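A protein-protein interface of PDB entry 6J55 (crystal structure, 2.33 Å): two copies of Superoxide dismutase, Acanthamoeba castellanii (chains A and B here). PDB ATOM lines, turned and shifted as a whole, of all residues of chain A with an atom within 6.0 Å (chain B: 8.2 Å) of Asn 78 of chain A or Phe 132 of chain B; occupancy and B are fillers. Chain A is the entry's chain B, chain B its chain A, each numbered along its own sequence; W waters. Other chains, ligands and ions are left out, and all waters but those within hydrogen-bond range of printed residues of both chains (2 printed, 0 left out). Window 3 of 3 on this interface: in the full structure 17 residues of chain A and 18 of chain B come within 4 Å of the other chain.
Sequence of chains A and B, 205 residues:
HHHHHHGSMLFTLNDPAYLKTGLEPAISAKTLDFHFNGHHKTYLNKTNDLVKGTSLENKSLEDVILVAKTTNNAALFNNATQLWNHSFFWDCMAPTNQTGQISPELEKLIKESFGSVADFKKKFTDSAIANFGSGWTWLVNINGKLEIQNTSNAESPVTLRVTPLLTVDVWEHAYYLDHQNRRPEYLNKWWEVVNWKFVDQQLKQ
The backbone carbonyl oxygen (O) of Gly 133 of chain B is in hydrogen-bond range of the guanidinium group (NH2) of Arg 183 of chain B, 3.2 Å away. The backbone carbonyl oxygen (O) of Ala 74 of chain A lies close to the side-chain amide nitrogen (ND2) of Asn 78 of chain A. The indole nitrogen of Trp 171 of chain A lies within hydrogen-bond range of the backbone carbonyl oxygen of Asn 153 of chain A (2.9 Å).
Among the printed residues, pairs that only touch across the chains: Asn 78 of chain A with Phe 132 of chain B (3.6 Å), Trp 171 of chain A with Phe 132 of chain B (3.6 Å), Trp 171 of chain A with Gly 133 of chain B (3.6 Å), Asn 153 of chain A with Phe 132 of chain B (3.7 Å), Asn 153 of chain A with Gly 133 of chain B (3.7 Å) and Ala 154 of chain A with Phe 132 of chain B (3.9 Å).
Asn 73 of chain A touches none of the printed residues of chain B. Of chain B, only Phe 132 (3.6 Å) comes within 4 Å of Asn 78 of chain A. Printed residues of chain B within 4 Å of Asn 153 of chain A: Phe 132 and Gly 133. Of the printed residues of chain B, Ala 154 of chain A touches Phe 132 (3.9 Å). Of the printed residues of chain B, Trp 171 of chain A touches Phe 132 and Gly 133. Of the printed residues of chain A, Phe 132 of chain B touches Asn 78 (3.6 Å), Asn 153 (3.7 Å), Ala 154 (3.9 Å) and Trp 171 (3.6 Å). Of the printed residues of chain A, Gly 133 of chain B touches Asn 153 (3.7 Å) and Trp 171 (3.6 Å). The nearest residue of chain B that does not touch Asn 78 of chain A is Ala 130 of chain B (6.6 Å). The nearest residue of chain A that does not touch Phe 132 of chain B is Gln 82 of chain A (4.1 Å). The nearest printed residue of chain B that does not touch Ala 154 of chain A is Gly 133 of chain B (7.2 Å).
Printed residues of chain B that touch a printed residue of chain A: Phe 132 and Gly 133. Hydrophobic or aromatic side chains of chain B within 4 Å of the printed part of chain A: Phe 132. Of the 16 printed residues of chain A, 4 touch a printed residue of chain B. Printed residues of chain A that touch a printed residue of chain B: Asn 78, Asn 153, Ala 154 and Trp 171. Hydrophobic or aromatic side chains of chain A within 4 Å of the printed part of chain B: Ala 154 and Trp 171.
Position printed for both chains: 153.
Water W2 lies within hydrogen-bond range of the side-chain amide oxygen of Asn 153 of chain A (2.4 Å), the side-chain amide oxygen of Asn 153 of chain B (2.7 Å) and the backbone NH of Ser 134 of chain B (3.1 Å). Water W1 lies within hydrogen-bond range of O of Phe 132 of chain B (2.7 Å), O of Ser 134 of chain B (2.8 Å), ND2 of Asn 153 of chain A (3.1 Å) and OG of Ser 152 of chain B (3.5 Å).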
ATOM      1  N   TYR A  43      -0.925 -24.693 -13.416  1.00  0.00           N
ATOM      2  CA  TYR A  43      -1.916 -25.209 -12.463  1.00  0.00           C
ATOM      3  C   TYR A  43      -1.737 -26.709 -12.220  1.00  0.00           C
ATOM      4  O   TYR A  43      -1.945 -27.190 -11.102  1.00  0.00           O
ATOM      5  CB  TYR A  43      -3.341 -24.922 -12.945  1.00  0.00           C
ATOM      6  CG  TYR A  43      -3.721 -23.463 -12.960  1.00  0.00           C
ATOM      7  CD1 TYR A  43      -4.383 -22.907 -14.062  1.00  0.00           C
ATOM      8  CD2 TYR A  43      -3.472 -22.647 -11.861  1.00  0.00           C
ATOM      9  CE1 TYR A  43      -4.759 -21.554 -14.081  1.00  0.00           C
ATOM     10  CE2 TYR A  43      -3.833 -21.292 -11.860  1.00  0.00           C
ATOM     11  CZ  TYR A  43      -4.475 -20.746 -12.967  1.00  0.00           C
ATOM     12  OH  TYR A  43      -4.832 -19.412 -12.960  1.00  0.00           O
ATOM     13  N   ALA A  68     -10.082 -29.423  -0.684  1.00  0.00           N
ATOM     14  CA  ALA A  68      -9.564 -28.061  -0.601  1.00  0.00           C
ATOM     15  C   ALA A  68     -10.660 -27.091  -0.176  1.00  0.00           C
ATOM     16  O   ALA A  68     -10.444 -26.209   0.666  1.00  0.00           O
ATOM     17  CB  ALA A  68      -8.984 -27.643  -1.952  1.00  0.00           C
ATOM     18  N   ASN A  73      -8.657 -24.612   1.997  1.00  0.00           N
ATOM     19  CA  ASN A  73      -7.255 -24.677   1.586  1.00  0.00           C
ATOM     20  C   ASN A  73      -7.157 -23.864   0.291  1.00  0.00           C
ATOM     21  O   ASN A  73      -7.508 -24.346  -0.783  1.00  0.00           O
ATOM     22  CB  ASN A  73      -6.825 -26.142   1.424  1.00  0.00           C
ATOM     23  CG  ASN A  73      -5.338 -26.306   1.203  1.00  0.00           C
ATOM     24  OD1 ASN A  73      -4.651 -25.415   0.700  1.00  0.00           O
ATOM     25  ND2 ASN A  73      -4.816 -27.433   1.646  1.00  0.00           N
ATOM     26  N   ALA A  74      -6.726 -22.607   0.408  1.00  0.00           N
ATOM     27  CA  ALA A  74      -6.826 -21.675  -0.717  1.00  0.00           C
ATOM     28  C   ALA A  74      -5.869 -22.050  -1.855  1.00  0.00           C
ATOM     29  O   ALA A  74      -6.279 -22.148  -3.019  1.00  0.00           O
ATOM     30  CB  ALA A  74      -6.587 -20.242  -0.221  1.00  0.00           C
ATOM     31  N   ALA A  75      -4.587 -22.263  -1.538  1.00  0.00           N
ATOM     32  CA  ALA A  75      -3.619 -22.615  -2.576  1.00  0.00           C
ATOM     33  C   ALA A  75      -4.004 -23.920  -3.277  1.00  0.00           C
ATOM     34  O   ALA A  75      -3.847 -24.048  -4.498  1.00  0.00           O
ATOM     35  CB  ALA A  75      -2.208 -22.689  -1.988  1.00  0.00           C
ATOM     36  N   LEU A  76      -4.497 -24.905  -2.531  1.00  0.00           N
ATOM     37  CA  LEU A  76      -4.895 -26.148  -3.182  1.00  0.00           C
ATOM     38  C   LEU A  76      -6.145 -25.960  -4.033  1.00  0.00           C
ATOM     39  O   LEU A  76      -6.206 -26.450  -5.166  1.00  0.00           O
ATOM     40  CB  LEU A  76      -5.106 -27.258  -2.143  1.00  0.00           C
ATOM     41  CG  LEU A  76      -5.574 -28.617  -2.686  1.00  0.00           C
ATOM     42  CD1 LEU A  76      -4.522 -29.183  -3.628  1.00  0.00           C
ATOM     43  CD2 LEU A  76      -5.862 -29.608  -1.544  1.00  0.00           C
ATOM     44  N   PHE A  77      -7.141 -25.237  -3.524  1.00  0.00           N
ATOM     45  CA  PHE A  77      -8.373 -25.048  -4.283  1.00  0.00           C
ATOM     46  C   PHE A  77      -8.120 -24.265  -5.578  1.00  0.00           C
ATOM     47  O   PHE A  77      -8.623 -24.623  -6.652  1.00  0.00           O
ATOM     48  CB  PHE A  77      -9.423 -24.334  -3.422  1.00  0.00           C
ATOM     49  CG  PHE A  77     -10.746 -24.175  -4.114  1.00  0.00           C
ATOM     50  CD1 PHE A  77     -11.652 -25.231  -4.145  1.00  0.00           C
ATOM     51  CD2 PHE A  77     -11.054 -23.005  -4.798  1.00  0.00           C
ATOM     52  CE1 PHE A  77     -12.863 -25.103  -4.799  1.00  0.00           C
ATOM     53  CE2 PHE A  77     -12.265 -22.877  -5.479  1.00  0.00           C
ATOM     54  CZ  PHE A  77     -13.168 -23.923  -5.477  1.00  0.00           C
ATOM     55  N   ASN A  78      -7.344 -23.190  -5.497  1.00  0.00           N
ATOM     56  CA  ASN A  78      -7.138 -22.363  -6.680  1.00  0.00           C
ATOM     57  C   ASN A  78      -6.469 -23.153  -7.798  1.00  0.00           C
ATOM     58  O   ASN A  78      -6.908 -23.099  -8.949  1.00  0.00           O
ATOM     59  CB  ASN A  78      -6.301 -21.131  -6.322  1.00  0.00           C
ATOM     60  CG  ASN A  78      -7.054 -20.165  -5.437  1.00  0.00           C
ATOM     61  OD1 ASN A  78      -8.289 -20.149  -5.435  1.00  0.00           O
ATOM     62  ND2 ASN A  78      -6.316 -19.324  -4.702  1.00  0.00           N
ATOM     63  N   ASN A  79      -5.444 -23.939  -7.471  1.00  0.00           N
ATOM     64  CA  ASN A  79      -4.713 -24.650  -8.518  1.00  0.00           C
ATOM     65  C   ASN A  79      -5.487 -25.856  -9.019  1.00  0.00           C
ATOM     66  O   ASN A  79      -5.630 -26.047 -10.227  1.00  0.00           O
ATOM     67  CB  ASN A  79      -3.331 -25.063  -8.011  1.00  0.00           C
ATOM     68  CG  ASN A  79      -2.390 -23.908  -7.936  1.00  0.00           C
ATOM     69  OD1 ASN A  79      -1.859 -23.472  -8.970  1.00  0.00           O
ATOM     70  ND2 ASN A  79      -2.192 -23.367  -6.732  1.00  0.00           N
ATOM     71  N   ALA A  80      -6.027 -26.653  -8.103  1.00  0.00           N
ATOM     72  CA  ALA A  80      -6.729 -27.863  -8.502  1.00  0.00           C
ATOM     73  C   ALA A  80      -7.990 -27.545  -9.286  1.00  0.00           C
ATOM     74  O   ALA A  80      -8.338 -28.265 -10.236  1.00  0.00           O
ATOM     75  CB  ALA A  80      -7.072 -28.700  -7.266  1.00  0.00           C
ATOM     76  N   THR A  81      -8.718 -26.496  -8.881  1.00  0.00           N
ATOM     77  CA  THR A  81      -9.974 -26.205  -9.560  1.00  0.00           C
ATOM     78  C   THR A  81      -9.720 -25.551 -10.908  1.00  0.00           C
ATOM     79  O   THR A  81     -10.430 -25.827 -11.887  1.00  0.00           O
ATOM     80  CB  THR A  81     -10.861 -25.327  -8.660  1.00  0.00           C
ATOM     81  OG1 THR A  81     -10.776 -25.800  -7.311  1.00  0.00           O
ATOM     82  CG2 THR A  81     -12.309 -25.426  -9.085  1.00  0.00           C
ATOM     83  N   GLN A  82      -8.704 -24.689 -10.985  1.00  0.00           N
ATOM     84  CA  GLN A  82      -8.296 -24.154 -12.282  1.00  0.00           C
ATOM     85  C   GLN A  82      -7.800 -25.256 -13.206  1.00  0.00           C
ATOM     86  O   GLN A  82      -8.012 -25.174 -14.426  1.00  0.00           O
ATOM     87  CB  GLN A  82      -7.214 -23.095 -12.108  1.00  0.00           C
ATOM     88  CG  GLN A  82      -7.730 -21.720 -11.639  1.00  0.00           C
ATOM     89  CD  GLN A  82      -8.606 -21.013 -12.638  1.00  0.00           C
ATOM     90  OE1 GLN A  82      -9.799 -21.297 -12.769  1.00  0.00           O
ATOM     91  NE2 GLN A  82      -8.001 -20.094 -13.384  1.00  0.00           N
ATOM     92  N   LEU A  83      -7.153 -26.304 -12.649  1.00  0.00           N
ATOM     93  CA  LEU A  83      -6.743 -27.434 -13.484  1.00  0.00           C
ATOM     94  C   LEU A  83      -7.954 -28.079 -14.141  1.00  0.00           C
ATOM     95  O   LEU A  83      -7.946 -28.336 -15.350  1.00  0.00           O
ATOM     96  CB  LEU A  83      -5.962 -28.460 -12.657  1.00  0.00           C
ATOM     97  CG  LEU A  83      -5.652 -29.838 -13.290  1.00  0.00           C
ATOM     98  CD1 LEU A  83      -4.771 -29.704 -14.525  1.00  0.00           C
ATOM     99  CD2 LEU A  83      -4.960 -30.768 -12.275  1.00  0.00           C
ATOM    100  N   ASN A 153     -12.625 -15.968 -10.046  1.00  0.00           N
ATOM    101  CA  ASN A 153     -11.289 -16.560  -9.935  1.00  0.00           C
ATOM    102  C   ASN A 153     -11.309 -18.061 -10.234  1.00  0.00           C
ATOM    103  O   ASN A 153     -11.453 -18.443 -11.400  1.00  0.00           O
ATOM    104  CB  ASN A 153     -10.677 -16.213  -8.572  1.00  0.00           C
ATOM    105  CG  ASN A 153     -10.382 -14.692  -8.431  1.00  0.00           C
ATOM    106  OD1 ASN A 153     -10.346 -13.974  -9.426  1.00  0.00           O
ATOM    107  ND2 ASN A 153     -10.207 -14.207  -7.200  1.00  0.00           N
ATOM    108  N   ALA A 154     -11.122 -18.928  -9.231  1.00  0.00           N
ATOM    109  CA  ALA A 154     -11.113 -20.361  -9.507  1.00  0.00           C
ATOM    110  C   ALA A 154     -12.441 -21.039  -9.219  1.00  0.00           C
ATOM    111  O   ALA A 154     -12.590 -22.207  -9.573  1.00  0.00           O
ATOM    112  CB  ALA A 154     -10.010 -21.077  -8.711  1.00  0.00           C
ATOM    113  N   TRP A 171     -11.110 -14.750 -17.435  1.00  0.00           N
ATOM    114  CA  TRP A 171      -9.802 -14.244 -17.057  1.00  0.00           C
ATOM    115  C   TRP A 171      -9.203 -13.518 -18.264  1.00  0.00           C
ATOM    116  O   TRP A 171      -9.377 -13.944 -19.420  1.00  0.00           O
ATOM    117  CB  TRP A 171      -8.870 -15.381 -16.610  1.00  0.00           C
ATOM    118  CG  TRP A 171      -9.042 -15.966 -15.200  1.00  0.00           C
ATOM    119  CD1 TRP A 171     -10.130 -16.627 -14.696  1.00  0.00           C
ATOM    120  CD2 TRP A 171      -8.049 -15.987 -14.159  1.00  0.00           C
ATOM    121  NE1 TRP A 171      -9.874 -17.048 -13.405  1.00  0.00           N
ATOM    122  CE2 TRP A 171      -8.608 -16.667 -13.055  1.00  0.00           C
ATOM    123  CE3 TRP A 171      -6.740 -15.497 -14.059  1.00  0.00           C
ATOM    124  CZ2 TRP A 171      -7.916 -16.843 -11.860  1.00  0.00           C
ATOM    125  CZ3 TRP A 171      -6.052 -15.675 -12.887  1.00  0.00           C
ATOM    126  CH2 TRP A 171      -6.638 -16.352 -11.792  1.00  0.00           C
ATOM    127  N   SER B 127       4.218 -10.804  -2.204  1.00  0.00           N
ATOM    128  CA  SER B 127       2.810 -10.570  -1.937  1.00  0.00           C
ATOM    129  C   SER B 127       2.039 -10.308  -3.230  1.00  0.00           C
ATOM    130  O   SER B 127       0.927 -10.817  -3.413  1.00  0.00           O
ATOM    131  CB  SER B 127       2.668  -9.397  -0.961  1.00  0.00           C
ATOM    132  OG  SER B 127       1.305  -9.120  -0.718  1.00  0.00           O
ATOM    133  N   ALA B 128       2.620  -9.516  -4.141  1.00  0.00           N
ATOM    134  CA  ALA B 128       1.959  -9.232  -5.413  1.00  0.00           C
ATOM    135  C   ALA B 128       1.840 -10.487  -6.276  1.00  0.00           C
ATOM    136  O   ALA B 128       0.816 -10.699  -6.932  1.00  0.00           O
ATOM    137  CB  ALA B 128       2.716  -8.130  -6.156  1.00  0.00           C
ATOM    138  N   ILE B 129       2.866 -11.341  -6.263  1.00  0.00           N
ATOM    139  CA  ILE B 129       2.817 -12.620  -6.980  1.00  0.00           C
ATOM    140  C   ILE B 129       1.742 -13.526  -6.397  1.00  0.00           C
ATOM    141  O   ILE B 129       1.002 -14.200  -7.130  1.00  0.00           O
ATOM    142  CB  ILE B 129       4.204 -13.295  -6.928  1.00  0.00           C
ATOM    143  CG1 ILE B 129       5.220 -12.508  -7.761  1.00  0.00           C
ATOM    144  CG2 ILE B 129       4.123 -14.780  -7.308  1.00  0.00           C
ATOM    145  CD1 ILE B 129       6.691 -12.983  -7.595  1.00  0.00           C
ATOM    146  N   ALA B 130       1.615 -13.539  -5.076  1.00  0.00           N
ATOM    147  CA  ALA B 130       0.666 -14.427  -4.414  1.00  0.00           C
ATOM    148  C   ALA B 130      -0.777 -13.965  -4.509  1.00  0.00           C
ATOM    149  O   ALA B 130      -1.680 -14.711  -4.115  1.00  0.00           O
ATOM    150  CB  ALA B 130       1.045 -14.556  -2.934  1.00  0.00           C
ATOM    151  N   ASN B 131      -1.020 -12.774  -5.030  1.00  0.00           N
ATOM    152  CA  ASN B 131      -2.356 -12.181  -5.104  1.00  0.00           C
ATOM    153  C   ASN B 131      -3.133 -12.822  -6.247  1.00  0.00           C
ATOM    154  O   ASN B 131      -2.930 -12.508  -7.422  1.00  0.00           O
ATOM    155  CB  ASN B 131      -2.236 -10.667  -5.238  1.00  0.00           C
ATOM    156  CG  ASN B 131      -3.519  -9.961  -4.953  1.00  0.00           C
ATOM    157  OD1 ASN B 131      -4.555 -10.590  -4.692  1.00  0.00           O
ATOM    158  ND2 ASN B 131      -3.458  -8.632  -4.935  1.00  0.00           N
ATOM    159  N   PHE B 132      -3.989 -13.766  -5.900  1.00  0.00           N
ATOM    160  CA  PHE B 132      -4.616 -14.605  -6.902  1.00  0.00           C
ATOM    161  C   PHE B 132      -5.709 -13.861  -7.654  1.00  0.00           C
ATOM    162  O   PHE B 132      -6.605 -13.261  -7.045  1.00  0.00           O
ATOM    163  CB  PHE B 132      -5.181 -15.869  -6.246  1.00  0.00           C
ATOM    164  CG  PHE B 132      -5.657 -16.880  -7.231  1.00  0.00           C
ATOM    165  CD1 PHE B 132      -4.738 -17.604  -7.993  1.00  0.00           C
ATOM    166  CD2 PHE B 132      -7.007 -17.125  -7.409  1.00  0.00           C
ATOM    167  CE1 PHE B 132      -5.165 -18.556  -8.917  1.00  0.00           C
ATOM    168  CE2 PHE B 132      -7.443 -18.090  -8.350  1.00  0.00           C
ATOM    169  CZ  PHE B 132      -6.526 -18.793  -9.092  1.00  0.00           C
ATOM    170  N   GLY B 133      -5.679 -13.966  -8.985  1.00  0.00           N
ATOM    171  CA  GLY B 133      -6.689 -13.298  -9.796  1.00  0.00           C
ATOM    172  C   GLY B 133      -6.334 -11.841 -10.040  1.00  0.00           C
ATOM    173  O   GLY B 133      -5.167 -11.465 -10.054  1.00  0.00           O
ATOM    174  N   SER B 134      -7.368 -11.023 -10.248  1.00  0.00           N
ATOM    175  CA  SER B 134      -7.222  -9.584 -10.464  1.00  0.00           C
ATOM    176  C   SER B 134      -7.159  -8.837  -9.139  1.00  0.00           C
ATOM    177  O   SER B 134      -7.899  -9.145  -8.198  1.00  0.00           O
ATOM    178  CB  SER B 134      -8.396  -9.027 -11.272  1.00  0.00           C
ATOM    179  OG  SER B 134      -8.580  -9.761 -12.464  1.00  0.00           O
ATOM    180  N   GLY B 135      -6.319  -7.807  -9.094  1.00  0.00           N
ATOM    181  CA  GLY B 135      -6.237  -7.014  -7.887  1.00  0.00           C
ATOM    182  C   GLY B 135      -5.003  -6.151  -7.855  1.00  0.00           C
ATOM    183  O   GLY B 135      -4.371  -5.877  -8.883  1.00  0.00           O
ATOM    184  N   TRP B 136      -4.676  -5.734  -6.644  1.00  0.00           N
ATOM    185  CA  TRP B 136      -3.657  -4.728  -6.421  1.00  0.00           C
ATOM    186  C   TRP B 136      -2.882  -5.068  -5.168  1.00  0.00           C
ATOM    187  O   TRP B 136      -3.431  -5.634  -4.223  1.00  0.00           O
ATOM    188  CB  TRP B 136      -4.288  -3.335  -6.232  1.00  0.00           C
ATOM    189  CG  TRP B 136      -5.205  -2.864  -7.329  1.00  0.00           C
ATOM    190  CD1 TRP B 136      -6.489  -3.244  -7.542  1.00  0.00           C
ATOM    191  CD2 TRP B 136      -4.898  -1.880  -8.342  1.00  0.00           C
ATOM    192  NE1 TRP B 136      -7.009  -2.563  -8.628  1.00  0.00           N
ATOM    193  CE2 TRP B 136      -6.050  -1.720  -9.131  1.00  0.00           C
ATOM    194  CE3 TRP B 136      -3.762  -1.125  -8.645  1.00  0.00           C
ATOM    195  CZ2 TRP B 136      -6.102  -0.839 -10.225  1.00  0.00           C
ATOM    196  CZ3 TRP B 136      -3.815  -0.243  -9.737  1.00  0.00           C
ATOM    197  CH2 TRP B 136      -4.981  -0.115 -10.511  1.00  0.00           C
ATOM    198  N   THR B 137      -1.615  -4.663  -5.144  1.00  0.00           N
ATOM    199  CA  THR B 137      -0.778  -4.778  -3.954  1.00  0.00           C
ATOM    200  C   THR B 137      -0.310  -3.380  -3.581  1.00  0.00           C
ATOM    201  O   THR B 137       0.109  -2.618  -4.457  1.00  0.00           O
ATOM    202  CB  THR B 137       0.408  -5.730  -4.190  1.00  0.00           C
ATOM    203  OG1 THR B 137      -0.093  -7.056  -4.357  1.00  0.00           O
ATOM    204  CG2 THR B 137       1.386  -5.716  -3.015  1.00  0.00           C
ATOM    205  N   ASN B 150      -2.703  -6.635   0.155  1.00  0.00           N
ATOM    206  CA  ASN B 150      -3.265  -7.152  -1.088  1.00  0.00           C
ATOM    207  C   ASN B 150      -4.764  -6.885  -1.136  1.00  0.00           C
ATOM    208  O   ASN B 150      -5.485  -7.153  -0.161  1.00  0.00           O
ATOM    209  CB  ASN B 150      -3.048  -8.657  -1.245  1.00  0.00           C
ATOM    210  CG  ASN B 150      -1.666  -9.021  -1.755  1.00  0.00           C
ATOM    211  OD1 ASN B 150      -0.812  -8.168  -2.011  1.00  0.00           O
ATOM    212  ND2 ASN B 150      -1.448 -10.327  -1.919  1.00  0.00           N
ATOM    213  N   THR B 151      -5.240  -6.404  -2.286  1.00  0.00           N
ATOM    214  CA  THR B 151      -6.667  -6.356  -2.539  1.00  0.00           C
ATOM    215  C   THR B 151      -6.981  -7.102  -3.828  1.00  0.00           C
ATOM    216  O   THR B 151      -6.132  -7.278  -4.703  1.00  0.00           O
ATOM    217  CB  THR B 151      -7.203  -4.914  -2.658  1.00  0.00           C
ATOM    218  OG1 THR B 151      -6.615  -4.262  -3.794  1.00  0.00           O
ATOM    219  CG2 THR B 151      -6.862  -4.134  -1.423  1.00  0.00           C
ATOM    220  N   SER B 152      -8.225  -7.525  -3.925  1.00  0.00           N
ATOM    221  CA  SER B 152      -8.733  -8.222  -5.088  1.00  0.00           C
ATOM    222  C   SER B 152      -9.668  -7.290  -5.870  1.00  0.00           C
ATOM    223  O   SER B 152     -10.433  -6.515  -5.275  1.00  0.00           O
ATOM    224  CB  SER B 152      -9.417  -9.519  -4.622  1.00  0.00           C
ATOM    225  OG  SER B 152     -10.766  -9.585  -4.993  1.00  0.00           O
ATOM    226  N   ASN B 153      -9.598  -7.365  -7.207  1.00  0.00           N
ATOM    227  CA  ASN B 153     -10.435  -6.600  -8.159  1.00  0.00           C
ATOM    228  C   ASN B 153     -10.333  -5.097  -7.936  1.00  0.00           C
ATOM    229  O   ASN B 153      -9.236  -4.526  -8.129  1.00  0.00           O
ATOM    230  CB  ASN B 153     -11.854  -7.189  -8.081  1.00  0.00           C
ATOM    231  CG  ASN B 153     -11.895  -8.646  -8.537  1.00  0.00           C
ATOM    232  OD1 ASN B 153     -10.928  -9.143  -9.094  1.00  0.00           O
ATOM    233  ND2 ASN B 153     -13.027  -9.310  -8.355  1.00  0.00           N
ATOM    234  N   VAL B 170      -1.990  -5.783 -10.573  1.00  0.00           N
ATOM    235  CA  VAL B 170      -1.730  -7.129 -11.066  1.00  0.00           C
ATOM    236  C   VAL B 170      -2.931  -7.747 -11.748  1.00  0.00           C
ATOM    237  O   VAL B 170      -2.933  -8.940 -12.021  1.00  0.00           O
ATOM    238  CB  VAL B 170      -1.163  -8.091  -9.988  1.00  0.00           C
ATOM    239  CG1 VAL B 170       0.055  -7.490  -9.301  1.00  0.00           C
ATOM    240  CG2 VAL B 170      -2.256  -8.435  -8.939  1.00  0.00           C
ATOM    241  N   ARG B 183       4.153 -12.858 -14.519  1.00  0.00           N
ATOM    242  CA  ARG B 183       3.987 -11.755 -13.578  1.00  0.00           C
ATOM    243  C   ARG B 183       5.239 -11.469 -12.770  1.00  0.00           C
ATOM    244  O   ARG B 183       5.541 -10.275 -12.569  1.00  0.00           O
ATOM    245  CB  ARG B 183       2.821 -12.034 -12.619  1.00  0.00           C
ATOM    246  CG  ARG B 183       2.395 -10.808 -11.775  1.00  0.00           C
ATOM    247  CD  ARG B 183       1.481 -11.213 -10.640  1.00  0.00           C
ATOM    248  NE  ARG B 183       0.147 -11.452 -11.147  1.00  0.00           N
ATOM    249  CZ  ARG B 183      -0.895 -11.724 -10.371  1.00  0.00           C
ATOM    250  NH1 ARG B 183      -0.735 -11.789  -9.055  1.00  0.00           N
ATOM    251  NH2 ARG B 183      -2.092 -11.922 -10.900  1.00  0.00           N
HETATM  252  O   HOH W   1      -8.647 -11.539  -6.977  1.00  0.00           O
HETATM  253  O   HOH W   2     -10.350 -11.623  -9.972  1.00  0.00           O
